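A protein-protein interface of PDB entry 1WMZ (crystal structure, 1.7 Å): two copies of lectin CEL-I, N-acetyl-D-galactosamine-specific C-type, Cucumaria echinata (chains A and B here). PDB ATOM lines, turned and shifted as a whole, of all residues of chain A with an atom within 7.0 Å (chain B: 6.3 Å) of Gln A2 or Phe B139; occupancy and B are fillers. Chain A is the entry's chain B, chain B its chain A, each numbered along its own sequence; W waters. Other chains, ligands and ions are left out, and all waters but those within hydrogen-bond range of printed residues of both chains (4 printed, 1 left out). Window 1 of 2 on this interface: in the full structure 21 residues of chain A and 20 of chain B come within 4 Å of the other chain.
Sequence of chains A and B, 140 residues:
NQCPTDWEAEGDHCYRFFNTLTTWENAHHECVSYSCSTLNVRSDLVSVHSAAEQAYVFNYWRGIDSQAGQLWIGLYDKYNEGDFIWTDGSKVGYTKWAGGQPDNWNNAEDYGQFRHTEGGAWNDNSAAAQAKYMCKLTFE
N of Gln B2 sits at hydrogen-bond distance from OE1 of Gln A2 (3.1 Å). The backbone carbonyl oxygen of Gly B11 sits at hydrogen-bond distance from the side-chain amide nitrogen of Gln A2 (2.8 Å). The backbone NH (N) of Asn A1 sits at hydrogen-bond distance from the side-chain carboxylate (OD1) of Asp B12 (3.3 Å). The backbone carbonyl oxygen (O) of Phe B139 lies within hydrogen-bond range of the side-chain hydroxyl (OG1) of Thr A5, 3.2 Å away. The chain-end carboxylate (O) of Glu B140 sits at hydrogen-bond distance from the side-chain hydroxyl (OG1) of Thr A5 (2.8 Å).
The side-chain amide oxygen (OD1) of Asn B1 lies within hydrogen-bond range of the backbone NH (N) of Cys B3 (2.9 Å). A ring nitrogen (ND1) of His B13 is in hydrogen-bond range of the backbone carbonyl oxygen (O) of Leu B137. The backbone NH of Leu B137 sits at hydrogen-bond distance from the backbone carbonyl oxygen of Cys B14 (2.8 Å). O of Asn B40 sits at hydrogen-bond distance from N of Glu B140 (3.0 Å). OE1 of Glu B140 lies within salt-bridge range of NE of Arg B42, 2.8 Å away. The backbone carbonyl oxygen (O) of Cys A14 lies within hydrogen-bond range of the backbone NH (N) of Leu A137 (2.9 Å).
Among the printed residues, merely in contact across the chains: Asn A1 with Gln B2 (3.3 Å), Gln A2 with Asn B1 (3.2 Å), Gln A2 with Cys B3 (3.7 Å), Gln A2 with Ala B9 (3.8 Å), Gln A2 with His B13 (3.6 Å), Gln A2 with Cys B14 (3.9 Å), Gln A2 with Phe B139 (3.1 Å), Cys A3 with Gln B2 (3.7 Å), Cys A3 with Phe B139 (3.7 Å), Pro A4 with Leu B39 (3.5 Å), Pro A4 with Phe B139 (3.8 Å), Ala A9 with Gln B2 (3.8 Å), Cys A14 with Gln B2 (3.8 Å), Leu A39 with Pro B4 (3.4 Å), Leu A39 with Val B41 (3.99 Å), Leu A137 with Leu B39 (3.9 Å), Phe A139 with Gln B2 (3.2 Å), Phe A139 with Cys B3 (3.8 Å) and Phe A139 with Pro B4 (3.9 Å).
Of chain B, only Asn B1 (3.2 Å), Gln B2 (3.1 Å), Cys B3 (3.7 Å), Ala B9 (3.8 Å), Gly B11 (2.8 Å), His B13 (3.6 Å), Cys B14 (3.9 Å) and Phe B139 (3.1 Å) come within 4 Å of Gln A2. Printed residues of chain A within 4 Å of Phe B139: Gln A2, Cys A3, Pro A4 and Thr A5. Printed residues of chain B within 4 Å of Phe A139: Gln B2, Cys B3 and Pro B4. Of the printed residues of chain B, Cys A3 touches Gln B2 (3.7 Å) and Phe B139 (3.7 Å). Of the printed residues of chain A, Pro B4 touches Leu A39 and Phe A139. Printed residues of chain A within 4 Å of Ala B9: Gln A2. Asn B40 touches none of the printed residues of chain A. Arg B42 touches none of the printed residues of chain A. The nearest printed residue of chain B that does not touch Gln A2 is Asp B12 (4.5 Å). The nearest printed residue of chain B that does not touch Leu A137 is Gln B2 (6.8 Å).
Of the 18 printed residues of chain B, 13 touch a printed residue of chain A. Hydrophobic or aromatic side chains of chain A within 4 Å of the printed part of chain B: Pro A4, Ala A9, Leu A39, Leu A137 and Phe A139. Among the printed residues, 24 pairs touch across the chains. Among the printed residues, no Asp or Glu carboxylate lies within 4 Å of a Lys or Arg side-chain nitrogen of the other chain.
Asn A1 touches Gln B2, and with the chains exchanged Gln A2 touches Asn B1. Gln A2 touches its own counterpart, Gln B2. Gln A2 touches Cys B3, and with the chains exchanged Cys A3 touches Gln B2. Gln A2 touches Ala B9, and with the chains exchanged Ala A9 touches Gln B2. Positions printed for both chains: 1, 2, 3, 4, 9, 14, 39, 137 and 139. Of the 24 pairs that touch across the chains among the printed residues, 17 have their exchanged pair printed and touching as well.
Water W3 bridges the side-chain hydroxyl (OG1) of Thr A5 (2.6 Å) and the backbone carbonyl oxygen (O) of Phe B139 (3.0 Å). Water W2 bridges O of Gln A2 (2.6 Å) and O of Gln B2 (2.7 Å). Water W1 lies within hydrogen-bond range of the backbone carbonyl oxygen (O) of Thr A5, the backbone carbonyl oxygen (O) of Leu B39 and the side-chain amide nitrogen (ND2) of Asn B40. Water W4 bridges the side-chain amide oxygen (OE1) of Gln A2 (2.9 Å) and the side-chain amide oxygen (OE1) of Gln B2 (2.9 Å).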
ATOM      1  N   ASN A   1       3.232  11.314  22.143  1.00  0.00           N
ATOM      2  CA  ASN A   1       2.086  12.257  21.952  1.00  0.00           C
ATOM      3  C   ASN A   1       0.751  11.508  22.000  1.00  0.00           C
ATOM      4  O   ASN A   1       0.706  10.287  22.188  1.00  0.00           O
ATOM      5  CB  ASN A   1       2.265  13.008  20.623  1.00  0.00           C
ATOM      6  CG  ASN A   1       2.305  12.066  19.428  1.00  0.00           C
ATOM      7  OD1 ASN A   1       1.370  11.313  19.208  1.00  0.00           O
ATOM      8  ND2 ASN A   1       3.371  12.129  18.644  1.00  0.00           N
ATOM      9  N   GLN A   2      -0.352  12.241  21.795  1.00  0.00           N
ATOM     10  CA  GLN A   2      -1.676  11.662  21.831  1.00  0.00           C
ATOM     11  C   GLN A   2      -2.396  11.612  20.467  1.00  0.00           C
ATOM     12  O   GLN A   2      -3.656  11.523  20.383  1.00  0.00           O
ATOM     13  CB  GLN A   2      -2.513  12.394  22.864  1.00  0.00           C
ATOM     14  CG  GLN A   2      -1.882  12.337  24.246  1.00  0.00           C
ATOM     15  CD  GLN A   2      -0.918  13.461  24.519  1.00  0.00           C
ATOM     16  OE1 GLN A   2      -1.105  14.552  24.032  1.00  0.00           O
ATOM     17  NE2 GLN A   2       0.138  13.178  25.291  1.00  0.00           N
ATOM     18  N   CYS A   3      -1.592  11.592  19.404  1.00  0.00           N
ATOM     19  CA  CYS A   3      -2.138  11.400  18.068  1.00  0.00           C
ATOM     20  C   CYS A   3      -2.420   9.940  17.779  1.00  0.00           C
ATOM     21  O   CYS A   3      -1.683   9.025  18.246  1.00  0.00           O
ATOM     22  CB  CYS A   3      -1.222  11.976  16.986  1.00  0.00           C
ATOM     23  SG  CYS A   3      -1.146  13.796  17.024  1.00  0.00           S
ATOM     24  N   PRO A   4      -3.457   9.694  16.987  1.00  0.00           N
ATOM     25  CA  PRO A   4      -3.701   8.350  16.446  1.00  0.00           C
ATOM     26  C   PRO A   4      -2.526   7.826  15.669  1.00  0.00           C
ATOM     27  O   PRO A   4      -1.693   8.591  15.166  1.00  0.00           O
ATOM     28  CB  PRO A   4      -4.911   8.551  15.534  1.00  0.00           C
ATOM     29  CG  PRO A   4      -5.625   9.770  16.145  1.00  0.00           C
ATOM     30  CD  PRO A   4      -4.499  10.666  16.583  1.00  0.00           C
ATOM     31  N   THR A   5      -2.414   6.508  15.655  1.00  0.00           N
ATOM     32  CA  THR A   5      -1.384   5.821  14.889  1.00  0.00           C
ATOM     33  C   THR A   5      -1.415   6.301  13.430  1.00  0.00           C
ATOM     34  O   THR A   5      -2.487   6.419  12.841  1.00  0.00           O
ATOM     35  CB  THR A   5      -1.650   4.341  14.999  1.00  0.00           C
ATOM     36  OG1 THR A   5      -1.581   4.013  16.386  1.00  0.00           O
ATOM     37  CG2 THR A   5      -0.598   3.481  14.198  1.00  0.00           C
ATOM     38  N   ALA A   9       2.256  14.524  15.466  1.00  0.00           N
ATOM     39  CA  ALA A   9       1.876  15.614  16.340  1.00  0.00           C
ATOM     40  C   ALA A   9       2.676  16.879  16.132  1.00  0.00           C
ATOM     41  O   ALA A   9       3.902  16.845  15.940  1.00  0.00           O
ATOM     42  CB  ALA A   9       2.045  15.172  17.768  1.00  0.00           C
ATOM     43  N   CYS A  14      -2.941  17.101  15.014  1.00  0.00           N
ATOM     44  CA  CYS A  14      -2.264  15.981  14.395  1.00  0.00           C
ATOM     45  C   CYS A  14      -2.379  16.135  12.881  1.00  0.00           C
ATOM     46  O   CYS A  14      -3.370  16.699  12.398  1.00  0.00           O
ATOM     47  CB  CYS A  14      -2.947  14.684  14.794  1.00  0.00           C
ATOM     48  SG  CYS A  14      -3.057  14.388  16.577  1.00  0.00           S
ATOM     49  N   LEU A  39     -15.718  12.001  19.949  1.00  0.00           N
ATOM     50  CA  LEU A  39     -14.633  12.696  20.630  1.00  0.00           C
ATOM     51  C   LEU A  39     -14.478  14.138  20.120  1.00  0.00           C
ATOM     52  O   LEU A  39     -13.565  14.845  20.514  1.00  0.00           O
ATOM     53  CB  LEU A  39     -13.329  11.901  20.421  1.00  0.00           C
ATOM     54  CG  LEU A  39     -13.294  10.499  21.050  1.00  0.00           C
ATOM     55  CD1 LEU A  39     -12.022   9.774  20.691  1.00  0.00           C
ATOM     56  CD2 LEU A  39     -13.420  10.612  22.509  1.00  0.00           C
ATOM     57  N   LEU A 137      -6.189  17.062  12.110  1.00  0.00           N
ATOM     58  CA  LEU A 137      -7.199  16.913  13.144  1.00  0.00           C
ATOM     59  C   LEU A 137      -7.273  18.143  14.002  1.00  0.00           C
ATOM     60  O   LEU A 137      -6.253  18.673  14.407  1.00  0.00           O
ATOM     61  CB  LEU A 137      -6.842  15.756  14.070  1.00  0.00           C
ATOM     62  CG  LEU A 137      -6.752  14.364  13.433  1.00  0.00           C
ATOM     63  CD1 LEU A 137      -6.624  13.294  14.501  1.00  0.00           C
ATOM     64  CD2 LEU A 137      -7.866  14.011  12.480  1.00  0.00           C
ATOM     65  N   PHE A 139      -9.276  19.323  17.478  1.00  0.00           N
ATOM     66  CA  PHE A 139     -10.032  18.845  18.642  1.00  0.00           C
ATOM     67  C   PHE A 139     -10.939  19.968  19.095  1.00  0.00           C
ATOM     68  O   PHE A 139     -10.539  20.857  19.805  1.00  0.00           O
ATOM     69  CB  PHE A 139      -9.061  18.398  19.713  1.00  0.00           C
ATOM     70  CG  PHE A 139      -8.127  17.343  19.208  1.00  0.00           C
ATOM     71  CD1 PHE A 139      -6.879  17.672  18.710  1.00  0.00           C
ATOM     72  CD2 PHE A 139      -8.549  16.030  19.125  1.00  0.00           C
ATOM     73  CE1 PHE A 139      -6.053  16.674  18.176  1.00  0.00           C
ATOM     74  CE2 PHE A 139      -7.727  15.039  18.603  1.00  0.00           C
ATOM     75  CZ  PHE A 139      -6.498  15.358  18.098  1.00  0.00           C
ATOM     76  N   ASN B   1      -1.325  19.605  24.151  1.00  0.00           N
ATOM     77  CA  ASN B   1      -1.524  18.150  23.903  1.00  0.00           C
ATOM     78  C   ASN B   1      -2.547  17.871  22.791  1.00  0.00           C
ATOM     79  O   ASN B   1      -3.223  18.769  22.301  1.00  0.00           O
ATOM     80  CB  ASN B   1      -1.942  17.444  25.206  1.00  0.00           C
ATOM     81  CG  ASN B   1      -3.387  17.832  25.688  1.00  0.00           C
ATOM     82  OD1 ASN B   1      -4.392  17.701  24.967  1.00  0.00           O
ATOM     83  ND2 ASN B   1      -3.469  18.287  26.935  1.00  0.00           N
ATOM     84  N   GLN B   2      -2.678  16.605  22.409  1.00  0.00           N
ATOM     85  CA  GLN B   2      -3.566  16.255  21.296  1.00  0.00           C
ATOM     86  C   GLN B   2      -4.784  15.460  21.752  1.00  0.00           C
ATOM     87  O   GLN B   2      -5.316  14.633  21.027  1.00  0.00           O
ATOM     88  CB  GLN B   2      -2.755  15.534  20.217  1.00  0.00           C
ATOM     89  CG  GLN B   2      -1.612  16.362  19.661  1.00  0.00           C
ATOM     90  CD  GLN B   2      -0.327  16.284  20.482  1.00  0.00           C
ATOM     91  OE1 GLN B   2      -0.041  15.263  21.099  1.00  0.00           O
ATOM     92  NE2 GLN B   2       0.457  17.341  20.456  1.00  0.00           N
ATOM     93  N   CYS B   3      -5.211  15.676  22.994  1.00  0.00           N
ATOM     94  CA  CYS B   3      -6.364  14.950  23.531  1.00  0.00           C
ATOM     95  C   CYS B   3      -7.635  15.649  23.124  1.00  0.00           C
ATOM     96  O   CYS B   3      -7.648  16.880  22.978  1.00  0.00           O
ATOM     97  CB  CYS B   3      -6.321  14.811  25.056  1.00  0.00           C
ATOM     98  SG  CYS B   3      -5.103  13.601  25.612  1.00  0.00           S
ATOM     99  N   PRO B   4      -8.696  14.890  22.876  1.00  0.00           N
ATOM    100  CA  PRO B   4     -10.017  15.484  22.724  1.00  0.00           C
ATOM    101  C   PRO B   4     -10.373  16.375  23.925  1.00  0.00           C
ATOM    102  O   PRO B   4      -9.851  16.183  25.025  1.00  0.00           O
ATOM    103  CB  PRO B   4     -10.943  14.285  22.647  1.00  0.00           C
ATOM    104  CG  PRO B   4     -10.063  13.203  22.027  1.00  0.00           C
ATOM    105  CD  PRO B   4      -8.708  13.437  22.635  1.00  0.00           C
ATOM    106  N   ALA B   9      -4.353  14.691  29.176  1.00  0.00           N
ATOM    107  CA  ALA B   9      -3.208  14.009  28.548  1.00  0.00           C
ATOM    108  C   ALA B   9      -2.191  13.504  29.580  1.00  0.00           C
ATOM    109  O   ALA B   9      -1.834  14.211  30.519  1.00  0.00           O
ATOM    110  CB  ALA B   9      -2.515  14.958  27.588  1.00  0.00           C
ATOM    111  N   GLU B  10      -1.674  12.312  29.364  1.00  0.00           N
ATOM    112  CA  GLU B  10      -0.545  11.824  30.137  1.00  0.00           C
ATOM    113  C   GLU B  10       0.083  10.709  29.326  1.00  0.00           C
ATOM    114  O   GLU B  10      -0.562   9.734  29.014  1.00  0.00           O
ATOM    115  CB  GLU B  10      -1.003  11.314  31.516  1.00  0.00           C
ATOM    116  CG  GLU B  10       0.101  10.767  32.410  1.00  0.00           C
ATOM    117  CD  GLU B  10       1.109  11.813  32.879  1.00  0.00           C
ATOM    118  OE1 GLU B  10       0.929  13.044  32.703  1.00  0.00           O
ATOM    119  OE2 GLU B  10       2.107  11.398  33.457  1.00  0.00           O
ATOM    120  N   GLY B  11       1.350  10.885  28.976  1.00  0.00           N
ATOM    121  CA  GLY B  11       2.086   9.895  28.218  1.00  0.00           C
ATOM    122  C   GLY B  11       1.424   9.764  26.878  1.00  0.00           C
ATOM    123  O   GLY B  11       1.027  10.761  26.289  1.00  0.00           O
ATOM    124  N   ASP B  12       1.278   8.533  26.398  1.00  0.00           N
ATOM    125  CA  ASP B  12       0.670   8.298  25.082  1.00  0.00           C
ATOM    126  C   ASP B  12      -0.852   8.046  25.184  1.00  0.00           C
ATOM    127  O   ASP B  12      -1.458   7.411  24.319  1.00  0.00           O
ATOM    128  CB  ASP B  12       1.387   7.127  24.423  1.00  0.00           C
ATOM    129  CG  ASP B  12       2.875   7.435  24.122  1.00  0.00           C
ATOM    130  OD1 ASP B  12       3.260   8.633  24.036  1.00  0.00           O
ATOM    131  OD2 ASP B  12       3.716   6.544  23.930  1.00  0.00           O
ATOM    132  N   HIS B  13      -1.480   8.579  26.226  1.00  0.00           N
ATOM    133  CA  HIS B  13      -2.913   8.293  26.479  1.00  0.00           C
ATOM    134  C   HIS B  13      -3.673   9.557  26.856  1.00  0.00           C
ATOM    135  O   HIS B  13      -3.054  10.549  27.198  1.00  0.00           O
ATOM    136  CB  HIS B  13      -3.057   7.240  27.597  1.00  0.00           C
ATOM    137  CG  HIS B  13      -2.521   5.883  27.224  1.00  0.00           C
ATOM    138  ND1 HIS B  13      -3.155   5.061  26.322  1.00  0.00           N
ATOM    139  CD2 HIS B  13      -1.411   5.217  27.622  1.00  0.00           C
ATOM    140  CE1 HIS B  13      -2.448   3.954  26.159  1.00  0.00           C
ATOM    141  NE2 HIS B  13      -1.383   4.019  26.937  1.00  0.00           N
ATOM    142  N   CYS B  14      -5.006   9.496  26.790  1.00  0.00           N
ATOM    143  CA  CYS B  14      -5.902  10.528  27.308  1.00  0.00           C
ATOM    144  C   CYS B  14      -6.793   9.842  28.332  1.00  0.00           C
ATOM    145  O   CYS B  14      -7.137   8.688  28.148  1.00  0.00           O
ATOM    146  CB  CYS B  14      -6.751  11.077  26.196  1.00  0.00           C
ATOM    147  SG  CYS B  14      -5.777  11.826  24.871  1.00  0.00           S
ATOM    148  N   LEU B  39     -10.237   6.453  13.388  1.00  0.00           N
ATOM    149  CA  LEU B  39      -8.876   6.806  13.811  1.00  0.00           C
ATOM    150  C   LEU B  39      -8.214   5.661  14.623  1.00  0.00           C
ATOM    151  O   LEU B  39      -7.149   5.857  15.186  1.00  0.00           O
ATOM    152  CB  LEU B  39      -8.901   8.067  14.663  1.00  0.00           C
ATOM    153  CG  LEU B  39      -9.159   9.344  13.830  1.00  0.00           C
ATOM    154  CD1 LEU B  39      -9.376  10.562  14.676  1.00  0.00           C
ATOM    155  CD2 LEU B  39      -8.048   9.560  12.862  1.00  0.00           C
ATOM    156  N   ASN B  40      -8.878   4.506  14.691  1.00  0.00           N
ATOM    157  CA  ASN B  40      -8.466   3.377  15.564  1.00  0.00           C
ATOM    158  C   ASN B  40      -8.183   3.813  16.982  1.00  0.00           C
ATOM    159  O   ASN B  40      -7.139   3.453  17.576  1.00  0.00           O
ATOM    160  CB  ASN B  40      -7.238   2.681  14.976  1.00  0.00           C
ATOM    161  CG  ASN B  40      -7.489   2.243  13.582  1.00  0.00           C
ATOM    162  OD1 ASN B  40      -8.320   1.381  13.357  1.00  0.00           O
ATOM    163  ND2 ASN B  40      -6.856   2.923  12.620  1.00  0.00           N
ATOM    164  N   VAL B  41      -9.079   4.648  17.501  1.00  0.00           N
ATOM    165  CA  VAL B  41      -9.038   5.047  18.893  1.00  0.00           C
ATOM    166  C   VAL B  41      -9.973   4.153  19.724  1.00  0.00           C
ATOM    167  O   VAL B  41     -11.201   4.219  19.623  1.00  0.00           O
ATOM    168  CB  VAL B  41      -9.428   6.528  19.101  1.00  0.00           C
ATOM    169  CG1 VAL B  41      -9.272   6.887  20.540  1.00  0.00           C
ATOM    170  CG2 VAL B  41      -8.567   7.506  18.224  1.00  0.00           C
ATOM    171  N   ARG B  42      -9.382   3.334  20.581  1.00  0.00           N
ATOM    172  CA  ARG B  42     -10.108   2.633  21.629  1.00  0.00           C
ATOM    173  C   ARG B  42     -10.350   3.533  22.845  1.00  0.00           C
ATOM    174  O   ARG B  42      -9.412   4.171  23.365  1.00  0.00           O
ATOM    175  CB  ARG B  42      -9.327   1.422  22.113  1.00  0.00           C
ATOM    176  CG  ARG B  42      -9.947   0.744  23.381  1.00  0.00           C
ATOM    177  CD  ARG B  42      -9.207  -0.506  23.864  1.00  0.00           C
ATOM    178  NE  ARG B  42      -9.321  -1.589  22.885  1.00  0.00           N
ATOM    179  CZ  ARG B  42     -10.295  -2.459  22.839  1.00  0.00           C
ATOM    180  NH1 ARG B  42     -11.236  -2.480  23.776  1.00  0.00           N
ATOM    181  NH2 ARG B  42     -10.330  -3.367  21.867  1.00  0.00           N
ATOM    182  N   LEU B 137      -8.136   6.567  26.620  1.00  0.00           N
ATOM    183  CA  LEU B 137      -7.991   6.366  25.169  1.00  0.00           C
ATOM    184  C   LEU B 137      -6.673   5.698  24.866  1.00  0.00           C
ATOM    185  O   LEU B 137      -5.648   6.102  25.403  1.00  0.00           O
ATOM    186  CB  LEU B 137      -8.030   7.678  24.396  1.00  0.00           C
ATOM    187  CG  LEU B 137      -9.276   8.567  24.563  1.00  0.00           C
ATOM    188  CD1 LEU B 137      -9.131   9.789  23.635  1.00  0.00           C
ATOM    189  CD2 LEU B 137     -10.538   7.812  24.299  1.00  0.00           C
ATOM    190  N   THR B 138      -6.726   4.715  23.988  1.00  0.00           N
ATOM    191  CA  THR B 138      -5.557   4.040  23.468  1.00  0.00           C
ATOM    192  C   THR B 138      -5.583   4.170  21.947  1.00  0.00           C
ATOM    193  O   THR B 138      -6.594   3.860  21.306  1.00  0.00           O
ATOM    194  CB  THR B 138      -5.569   2.581  23.827  1.00  0.00           C
ATOM    195  OG1 THR B 138      -5.560   2.399  25.263  1.00  0.00           O
ATOM    196  CG2 THR B 138      -4.296   1.914  23.327  1.00  0.00           C
ATOM    197  N   PHE B 139      -4.488   4.683  21.402  1.00  0.00           N
ATOM    198  CA  PHE B 139      -4.310   4.873  19.986  1.00  0.00           C
ATOM    199  C   PHE B 139      -3.712   3.609  19.390  1.00  0.00           C
ATOM    200  O   PHE B 139      -2.498   3.392  19.425  1.00  0.00           O
ATOM    201  CB  PHE B 139      -3.457   6.126  19.754  1.00  0.00           C
ATOM    202  CG  PHE B 139      -4.050   7.300  20.435  1.00  0.00           C
ATOM    203  CD1 PHE B 139      -3.525   7.777  21.619  1.00  0.00           C
ATOM    204  CD2 PHE B 139      -5.217   7.873  19.943  1.00  0.00           C
ATOM    205  CE1 PHE B 139      -4.137   8.818  22.293  1.00  0.00           C
ATOM    206  CE2 PHE B 139      -5.831   8.908  20.632  1.00  0.00           C
ATOM    207  CZ  PHE B 139      -5.293   9.372  21.797  1.00  0.00           C
ATOM    208  N   GLU B 140      -4.611   2.742  18.935  1.00  0.00           N
ATOM    209  CA  GLU B 140      -4.283   1.401  18.445  1.00  0.00           C
ATOM    210  C   GLU B 140      -3.778   1.348  17.023  1.00  0.00           C
ATOM    211  O   GLU B 140      -3.804   2.328  16.291  1.00  0.00           O
ATOM    212  CB  GLU B 140      -5.515   0.500  18.555  1.00  0.00           C
ATOM    213  CG  GLU B 140      -6.011   0.419  19.996  1.00  0.00           C
ATOM    214  CD  GLU B 140      -7.043  -0.658  20.210  1.00  0.00           C
ATOM    215  OE1 GLU B 140      -7.005  -1.307  21.280  1.00  0.00           O
ATOM    216  OE2 GLU B 140      -7.881  -0.877  19.335  1.00  0.00           O
ATOM    217  OXT GLU B 140      -3.297   0.303  16.504  1.00  0.00           O
HETATM  218  O   HOH W   1      -5.105   5.677  13.275  1.00  0.00           O
HETATM  219  O   HOH W   2      -6.097  12.324  19.863  1.00  0.00           O
HETATM  220  O   HOH W   3      -0.049   4.796  18.361  1.00  0.00           O
HETATM  221  O   HOH W   4       1.546  15.695  23.533  1.00  0.00           O
